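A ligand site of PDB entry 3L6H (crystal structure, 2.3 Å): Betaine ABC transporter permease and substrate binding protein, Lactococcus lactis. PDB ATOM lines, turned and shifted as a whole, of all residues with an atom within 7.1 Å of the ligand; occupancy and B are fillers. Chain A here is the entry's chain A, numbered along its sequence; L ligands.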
ATOM      1  N   MET A   9     -19.488   9.786  -7.370  1.00  0.00           N
ATOM      2  CA  MET A   9     -20.644   9.217  -8.062  1.00  0.00           C
ATOM      3  C   MET A   9     -20.251   7.963  -8.846  1.00  0.00           C
ATOM      4  O   MET A   9     -19.075   7.737  -9.114  1.00  0.00           O
ATOM      5  CB  MET A   9     -21.259  10.241  -9.020  1.00  0.00           C
ATOM      6  CG  MET A   9     -21.716  11.533  -8.357  1.00  0.00           C
ATOM      7  SD  MET A   9     -20.360  12.608  -7.839  1.00  0.00           S
ATOM      8  CE  MET A   9     -21.109  14.218  -8.085  1.00  0.00           C
ATOM      9  N   TRP A  11     -19.853   6.800 -11.850  1.00  0.00           N
ATOM     10  CA  TRP A  11     -19.443   6.895 -13.248  1.00  0.00           C
ATOM     11  C   TRP A  11     -18.001   6.409 -13.301  1.00  0.00           C
ATOM     12  O   TRP A  11     -17.221   6.710 -12.408  1.00  0.00           O
ATOM     13  CB  TRP A  11     -19.556   8.338 -13.758  1.00  0.00           C
ATOM     14  CG  TRP A  11     -20.878   8.970 -13.472  1.00  0.00           C
ATOM     15  CD1 TRP A  11     -22.108   8.436 -13.724  1.00  0.00           C
ATOM     16  CD2 TRP A  11     -21.121  10.241 -12.864  1.00  0.00           C
ATOM     17  NE1 TRP A  11     -23.097   9.300 -13.327  1.00  0.00           N
ATOM     18  CE2 TRP A  11     -22.515  10.422 -12.785  1.00  0.00           C
ATOM     19  CE3 TRP A  11     -20.280  11.256 -12.372  1.00  0.00           C
ATOM     20  CZ2 TRP A  11     -23.097  11.569 -12.248  1.00  0.00           C
ATOM     21  CZ3 TRP A  11     -20.860  12.394 -11.830  1.00  0.00           C
ATOM     22  CH2 TRP A  11     -22.252  12.543 -11.772  1.00  0.00           C
ATOM     23  N   ASP A  12     -17.663   5.659 -14.352  1.00  0.00           N
ATOM     24  CA  ASP A  12     -16.327   5.057 -14.455  1.00  0.00           C
ATOM     25  C   ASP A  12     -15.209   6.097 -14.295  1.00  0.00           C
ATOM     26  O   ASP A  12     -14.155   5.791 -13.732  1.00  0.00           O
ATOM     27  CB  ASP A  12     -16.167   4.322 -15.797  1.00  0.00           C
ATOM     28  CG  ASP A  12     -17.003   3.039 -15.868  1.00  0.00           C
ATOM     29  OD1 ASP A  12     -17.102   2.313 -14.857  1.00  0.00           O
ATOM     30  OD2 ASP A  12     -17.582   2.769 -16.947  1.00  0.00           O
ATOM     31  N   SER A  13     -15.455   7.311 -14.779  1.00  0.00           N
ATOM     32  CA  SER A  13     -14.505   8.414 -14.657  1.00  0.00           C
ATOM     33  C   SER A  13     -14.205   8.785 -13.196  1.00  0.00           C
ATOM     34  O   SER A  13     -13.045   8.983 -12.845  1.00  0.00           O
ATOM     35  CB  SER A  13     -14.991   9.642 -15.437  1.00  0.00           C
ATOM     36  OG  SER A  13     -16.368   9.888 -15.226  1.00  0.00           O
ATOM     37  N   GLU A  14     -15.241   8.853 -12.365  1.00  0.00           N
ATOM     38  CA  GLU A  14     -15.079   9.285 -10.971  1.00  0.00           C
ATOM     39  C   GLU A  14     -14.617   8.159 -10.045  1.00  0.00           C
ATOM     40  O   GLU A  14     -14.067   8.428  -8.975  1.00  0.00           O
ATOM     41  CB  GLU A  14     -16.371   9.891 -10.408  1.00  0.00           C
ATOM     42  CG  GLU A  14     -17.115  10.839 -11.335  1.00  0.00           C
ATOM     43  CD  GLU A  14     -16.228  11.815 -12.083  1.00  0.00           C
ATOM     44  OE1 GLU A  14     -15.336  12.426 -11.453  1.00  0.00           O
ATOM     45  OE2 GLU A  14     -16.416  11.970 -13.301  1.00  0.00           O
ATOM     46  N   ASN A  39     -25.657  11.901  -7.975  1.00  0.00           N
ATOM     47  CA  ASN A  39     -25.158  13.253  -8.259  1.00  0.00           C
ATOM     48  C   ASN A  39     -25.638  14.301  -7.254  1.00  0.00           C
ATOM     49  O   ASN A  39     -24.827  14.881  -6.532  1.00  0.00           O
ATOM     50  CB  ASN A  39     -25.561  13.641  -9.690  1.00  0.00           C
ATOM     51  CG  ASN A  39     -25.055  15.010 -10.094  1.00  0.00           C
ATOM     52  OD1 ASN A  39     -24.063  15.507  -9.565  1.00  0.00           O
ATOM     53  ND2 ASN A  39     -25.743  15.634 -11.042  1.00  0.00           N
ATOM     54  N   SER A  56     -15.472  15.578  -8.416  1.00  0.00           N
ATOM     55  CA  SER A  56     -16.320  15.125  -9.516  1.00  0.00           C
ATOM     56  C   SER A  56     -17.403  16.139  -9.913  1.00  0.00           C
ATOM     57  O   SER A  56     -18.513  15.757 -10.278  1.00  0.00           O
ATOM     58  CB  SER A  56     -16.946  13.788  -9.130  1.00  0.00           C
ATOM     59  OG  SER A  56     -17.611  13.883  -7.881  1.00  0.00           O
ATOM     60  N   TRP A  58     -18.674  18.444 -12.602  1.00  0.00           N
ATOM     61  CA  TRP A  58     -18.601  18.756 -14.029  1.00  0.00           C
ATOM     62  C   TRP A  58     -19.267  20.103 -14.283  1.00  0.00           C
ATOM     63  O   TRP A  58     -20.498  20.214 -14.252  1.00  0.00           O
ATOM     64  CB  TRP A  58     -19.282  17.660 -14.847  1.00  0.00           C
ATOM     65  CG  TRP A  58     -18.511  16.384 -14.895  1.00  0.00           C
ATOM     66  CD1 TRP A  58     -18.158  15.602 -13.840  1.00  0.00           C
ATOM     67  CD2 TRP A  58     -18.000  15.740 -16.072  1.00  0.00           C
ATOM     68  NE1 TRP A  58     -17.452  14.506 -14.283  1.00  0.00           N
ATOM     69  CE2 TRP A  58     -17.335  14.561 -15.649  1.00  0.00           C
ATOM     70  CE3 TRP A  58     -18.042  16.039 -17.440  1.00  0.00           C
ATOM     71  CZ2 TRP A  58     -16.718  13.690 -16.542  1.00  0.00           C
ATOM     72  CZ3 TRP A  58     -17.420  15.174 -18.325  1.00  0.00           C
ATOM     73  CH2 TRP A  58     -16.773  14.002 -17.871  1.00  0.00           C
ATOM     74  N   THR A  62     -22.726  20.915 -17.225  1.00  0.00           N
ATOM     75  CA  THR A  62     -23.198  19.561 -16.916  1.00  0.00           C
ATOM     76  C   THR A  62     -23.930  19.500 -15.581  1.00  0.00           C
ATOM     77  O   THR A  62     -25.015  18.936 -15.501  1.00  0.00           O
ATOM     78  CB  THR A  62     -22.053  18.542 -16.958  1.00  0.00           C
ATOM     79  OG1 THR A  62     -21.441  18.577 -18.261  1.00  0.00           O
ATOM     80  CG2 THR A  62     -22.563  17.126 -16.680  1.00  0.00           C
ATOM     81  N   HIS A  63     -23.358  20.111 -14.534  1.00  0.00           N
ATOM     82  CA  HIS A  63     -23.995  20.124 -13.208  1.00  0.00           C
ATOM     83  C   HIS A  63     -24.526  21.515 -12.830  1.00  0.00           C
ATOM     84  O   HIS A  63     -24.447  21.916 -11.672  1.00  0.00           O
ATOM     85  CB  HIS A  63     -23.023  19.635 -12.125  1.00  0.00           C
ATOM     86  CG  HIS A  63     -22.711  18.172 -12.216  1.00  0.00           C
ATOM     87  ND1 HIS A  63     -21.627  17.605 -11.593  1.00  0.00           N
ATOM     88  CD2 HIS A  63     -23.342  17.158 -12.865  1.00  0.00           C
ATOM     89  CE1 HIS A  63     -21.597  16.308 -11.841  1.00  0.00           C
ATOM     90  NE2 HIS A  63     -22.621  16.013 -12.613  1.00  0.00           N
ATOM     91  N   LYS A  85     -15.720  16.687 -21.958  1.00  0.00           N
ATOM     92  CA  LYS A  85     -16.882  16.968 -22.799  1.00  0.00           C
ATOM     93  C   LYS A  85     -18.019  15.975 -22.638  1.00  0.00           C
ATOM     94  O   LYS A  85     -17.815  14.843 -22.195  1.00  0.00           O
ATOM     95  CB  LYS A  85     -16.476  17.070 -24.279  1.00  0.00           C
ATOM     96  CG  LYS A  85     -15.477  16.036 -24.756  1.00  0.00           C
ATOM     97  CD  LYS A  85     -15.141  16.245 -26.225  1.00  0.00           C
ATOM     98  CE  LYS A  85     -13.769  15.670 -26.577  1.00  0.00           C
ATOM     99  NZ  LYS A  85     -12.651  16.543 -26.124  1.00  0.00           N
ATOM    100  N   VAL A  86     -19.204  16.435 -23.015  1.00  0.00           N
ATOM    101  CA  VAL A  86     -20.439  15.653 -22.973  1.00  0.00           C
ATOM    102  C   VAL A  86     -21.120  15.834 -24.324  1.00  0.00           C
ATOM    103  O   VAL A  86     -20.959  16.874 -24.967  1.00  0.00           O
ATOM    104  CB  VAL A  86     -21.350  16.196 -21.847  1.00  0.00           C
ATOM    105  CG1 VAL A  86     -22.772  15.685 -22.006  1.00  0.00           C
ATOM    106  CG2 VAL A  86     -20.799  15.817 -20.480  1.00  0.00           C
ATOM    107  N   ILE A 113     -28.259   7.373 -19.297  1.00  0.00           N
ATOM    108  CA  ILE A 113     -27.787   6.741 -18.050  1.00  0.00           C
ATOM    109  C   ILE A 113     -28.826   7.008 -16.952  1.00  0.00           C
ATOM    110  O   ILE A 113     -30.002   7.164 -17.271  1.00  0.00           O
ATOM    111  CB  ILE A 113     -26.362   7.223 -17.677  1.00  0.00           C
ATOM    112  CG1 ILE A 113     -26.315   8.749 -17.489  1.00  0.00           C
ATOM    113  CG2 ILE A 113     -25.372   6.785 -18.758  1.00  0.00           C
ATOM    114  CD1 ILE A 113     -24.930   9.273 -17.120  1.00  0.00           C
ATOM    115  N   GLU A 114     -28.415   7.036 -15.675  1.00  0.00           N
ATOM    116  CA  GLU A 114     -29.386   7.241 -14.588  1.00  0.00           C
ATOM    117  C   GLU A 114     -30.006   8.639 -14.664  1.00  0.00           C
ATOM    118  O   GLU A 114     -29.325   9.586 -15.039  1.00  0.00           O
ATOM    119  CB  GLU A 114     -28.761   6.977 -13.203  1.00  0.00           C
ATOM    120  CG  GLU A 114     -27.921   8.118 -12.582  1.00  0.00           C
ATOM    121  CD  GLU A 114     -26.550   8.275 -13.220  1.00  0.00           C
ATOM    122  OE1 GLU A 114     -25.813   9.204 -12.812  1.00  0.00           O
ATOM    123  OE2 GLU A 114     -26.193   7.465 -14.111  1.00  0.00           O
ATOM    124  N   GLY A 116     -30.708  11.107 -12.789  1.00  0.00           N
ATOM    125  CA  GLY A 116     -30.168  12.232 -12.028  1.00  0.00           C
ATOM    126  C   GLY A 116     -28.869  12.833 -12.543  1.00  0.00           C
ATOM    127  O   GLY A 116     -28.438  13.871 -12.046  1.00  0.00           O
ATOM    128  N   ALA A 117     -28.242  12.200 -13.529  1.00  0.00           N
ATOM    129  CA  ALA A 117     -26.966  12.687 -14.075  1.00  0.00           C
ATOM    130  C   ALA A 117     -27.155  14.010 -14.820  1.00  0.00           C
ATOM    131  O   ALA A 117     -28.217  14.270 -15.402  1.00  0.00           O
ATOM    132  CB  ALA A 117     -26.346  11.651 -14.982  1.00  0.00           C
ATOM    133  N   GLY A 118     -26.122  14.853 -14.801  1.00  0.00           N
ATOM    134  CA  GLY A 118     -26.153  16.144 -15.483  1.00  0.00           C
ATOM    135  C   GLY A 118     -26.300  16.070 -16.986  1.00  0.00           C
ATOM    136  O   GLY A 118     -26.906  16.942 -17.599  1.00  0.00           O
ATOM    137  N   VAL A 119     -25.737  15.015 -17.584  1.00  0.00           N
ATOM    138  CA  VAL A 119     -25.806  14.809 -19.032  1.00  0.00           C
ATOM    139  C   VAL A 119     -27.241  14.545 -19.475  1.00  0.00           C
ATOM    140  O   VAL A 119     -27.609  14.850 -20.608  1.00  0.00           O
ATOM    141  CB  VAL A 119     -24.893  13.638 -19.491  1.00  0.00           C
ATOM    142  CG1 VAL A 119     -25.363  12.305 -18.907  1.00  0.00           C
ATOM    143  CG2 VAL A 119     -24.833  13.562 -21.003  1.00  0.00           C
ATOM    144  N   MET A 120     -28.051  13.998 -18.573  1.00  0.00           N
ATOM    145  CA  MET A 120     -29.464  13.728 -18.865  1.00  0.00           C
ATOM    146  C   MET A 120     -30.265  15.027 -18.921  1.00  0.00           C
ATOM    147  O   MET A 120     -31.101  15.197 -19.796  1.00  0.00           O
ATOM    148  CB  MET A 120     -30.050  12.778 -17.831  1.00  0.00           C
ATOM    149  CG  MET A 120     -29.391  11.410 -17.822  1.00  0.00           C
ATOM    150  SD  MET A 120     -29.729  10.448 -19.315  1.00  0.00           S
ATOM    151  CE  MET A 120     -31.446   9.992 -19.027  1.00  0.00           C
ATOM    152  N   ALA A 121     -30.012  15.941 -17.980  1.00  0.00           N
ATOM    153  CA  ALA A 121     -30.644  17.262 -17.987  1.00  0.00           C
ATOM    154  C   ALA A 121     -30.301  18.030 -19.267  1.00  0.00           C
ATOM    155  O   ALA A 121     -31.180  18.639 -19.875  1.00  0.00           O
ATOM    156  CB  ALA A 121     -30.219  18.065 -16.756  1.00  0.00           C
ATOM    157  N   SER A 143     -25.166   3.871 -16.155  1.00  0.00           N
ATOM    158  CA  SER A 143     -23.819   3.911 -16.730  1.00  0.00           C
ATOM    159  C   SER A 143     -23.413   2.588 -17.345  1.00  0.00           C
ATOM    160  O   SER A 143     -22.973   2.540 -18.497  1.00  0.00           O
ATOM    161  CB  SER A 143     -22.806   4.281 -15.657  1.00  0.00           C
ATOM    162  OG  SER A 143     -23.021   5.589 -15.193  1.00  0.00           O
ATOM    163  N   THR A 163     -25.843   8.987 -24.596  1.00  0.00           N
ATOM    164  CA  THR A 163     -25.372  10.125 -23.831  1.00  0.00           C
ATOM    165  C   THR A 163     -23.946   9.823 -23.388  1.00  0.00           C
ATOM    166  O   THR A 163     -23.739   9.205 -22.343  1.00  0.00           O
ATOM    167  CB  THR A 163     -26.258  10.379 -22.599  1.00  0.00           C
ATOM    168  OG1 THR A 163     -26.325   9.177 -21.800  1.00  0.00           O
ATOM    169  CG2 THR A 163     -27.662  10.781 -23.014  1.00  0.00           C
ATOM    170  N   GLY A 164     -22.982  10.230 -24.207  1.00  0.00           N
ATOM    171  CA  GLY A 164     -21.584   9.933 -23.963  1.00  0.00           C
ATOM    172  C   GLY A 164     -20.831  11.099 -23.348  1.00  0.00           C
ATOM    173  O   GLY A 164     -21.351  12.205 -23.253  1.00  0.00           O
ATOM    174  N   TRP A 165     -19.611  10.827 -22.913  1.00  0.00           N
ATOM    175  CA  TRP A 165     -18.735  11.858 -22.360  1.00  0.00           C
ATOM    176  C   TRP A 165     -17.279  11.418 -22.424  1.00  0.00           C
ATOM    177  O   TRP A 165     -16.979  10.232 -22.580  1.00  0.00           O
ATOM    178  CB  TRP A 165     -19.123  12.169 -20.919  1.00  0.00           C
ATOM    179  CG  TRP A 165     -18.900  11.031 -19.944  1.00  0.00           C
ATOM    180  CD1 TRP A 165     -17.777  10.796 -19.202  1.00  0.00           C
ATOM    181  CD2 TRP A 165     -19.835  10.011 -19.589  1.00  0.00           C
ATOM    182  NE1 TRP A 165     -17.944   9.689 -18.421  1.00  0.00           N
ATOM    183  CE2 TRP A 165     -19.202   9.185 -18.638  1.00  0.00           C
ATOM    184  CE3 TRP A 165     -21.144   9.707 -19.984  1.00  0.00           C
ATOM    185  CZ2 TRP A 165     -19.840   8.073 -18.075  1.00  0.00           C
ATOM    186  CZ3 TRP A 165     -21.764   8.610 -19.428  1.00  0.00           C
ATOM    187  CH2 TRP A 165     -21.113   7.799 -18.483  1.00  0.00           C
ATOM    188  N   SER A 166     -16.380  12.392 -22.321  1.00  0.00           N
ATOM    189  CA  SER A 166     -14.942  12.149 -22.239  1.00  0.00           C
ATOM    190  C   SER A 166     -14.431  12.825 -20.975  1.00  0.00           C
ATOM    191  O   SER A 166     -14.877  13.926 -20.643  1.00  0.00           O
ATOM    192  CB  SER A 166     -14.236  12.734 -23.462  1.00  0.00           C
ATOM    193  OG  SER A 166     -14.712  12.147 -24.658  1.00  0.00           O
ATOM    194  N   PRO A 167     -13.477  12.196 -20.265  1.00  0.00           N
ATOM    195  CA  PRO A 167     -12.808  10.928 -20.577  1.00  0.00           C
ATOM    196  C   PRO A 167     -13.657   9.675 -20.318  1.00  0.00           C
ATOM    197  O   PRO A 167     -14.420   9.625 -19.342  1.00  0.00           O
ATOM    198  CB  PRO A 167     -11.581  10.935 -19.655  1.00  0.00           C
ATOM    199  CG  PRO A 167     -11.492  12.316 -19.106  1.00  0.00           C
ATOM    200  CD  PRO A 167     -12.883  12.814 -19.064  1.00  0.00           C
ATOM    201  N   ILE A 192     -13.676  19.129 -15.218  1.00  0.00           N
ATOM    202  CA  ILE A 192     -13.985  18.425 -13.972  1.00  0.00           C
ATOM    203  C   ILE A 192     -13.352  19.221 -12.841  1.00  0.00           C
ATOM    204  O   ILE A 192     -12.169  19.550 -12.903  1.00  0.00           O
ATOM    205  CB  ILE A 192     -13.441  16.991 -13.947  1.00  0.00           C
ATOM    206  CG1 ILE A 192     -13.843  16.224 -15.215  1.00  0.00           C
ATOM    207  CG2 ILE A 192     -13.942  16.264 -12.710  1.00  0.00           C
ATOM    208  CD1 ILE A 192     -13.480  14.753 -15.184  1.00  0.00           C
HETATM  209  N1  LIG L   1     -20.982  12.359 -16.319  1.00  0.00           N
HETATM  210  C1  LIG L   1     -21.460  13.322 -15.301  1.00  0.00           C
HETATM  211  C2  LIG L   1     -22.916  13.716 -15.417  1.00  0.00           C
HETATM  212  O1  LIG L   1     -23.516  13.613 -16.513  1.00  0.00           O
HETATM  213  O2  LIG L   1     -23.483  14.130 -14.376  1.00  0.00           O
HETATM  214  C3  LIG L   1     -19.697  11.796 -15.866  1.00  0.00           C
HETATM  215  C4  LIG L   1     -20.763  13.051 -17.600  1.00  0.00           C
HETATM  216  C5  LIG L   1     -21.926  11.251 -16.509  1.00  0.00           C
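The backbone carbonyl oxygen of Trp 58 is in hydrogen-bond range of the backbone NH of His 63, 2.9 Å away.
The side-chain amide oxygen of Asn 39 sits at hydrogen-bond distance from a ring nitrogen (NE2) of His 63, at 3.4 Å.
NE1 of Trp 11 lies within hydrogen-bond range of OE1 of Glu 114 (2.8 Å).
OE2 of Glu 14 lies within hydrogen-bond range of NE1 of Trp 58, at 2.9 Å.
SD of Met 120 is in hydrogen-bond range of N of Ile 113, 3.4 Å away.
The side-chain hydroxyl (OG) of Ser 13 is in hydrogen-bond range of the side-chain carboxylate (OE2) of Glu 14, 2.8 Å away.
NE2 of His 63 is in hydrogen-bond range of O2 of the ligand (2.7 Å).
O2 of the ligand sits at hydrogen-bond distance from N of Gly 118 (2.8 Å).
N of Val 119 lies within hydrogen-bond range of O1 of the ligand (2.8 Å).
Residues that only touch the ligand: Trp 11, Trp 58, Trp 165, Thr 62, Ile 113, Ala 117, Ser 13 and Val 86.
Hydrophobic or aromatic side chains within 4 Å of the ligand: Trp 11, Trp 58, His 63, Val 86, Ile 113, Ala 117, Val 119 and Trp 165.
Along chain A the residues within 4 Å of the ligand span positions 11 to 165.
The nearest printed residue that does not touch the ligand is Glu 14 (4.2 Å).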
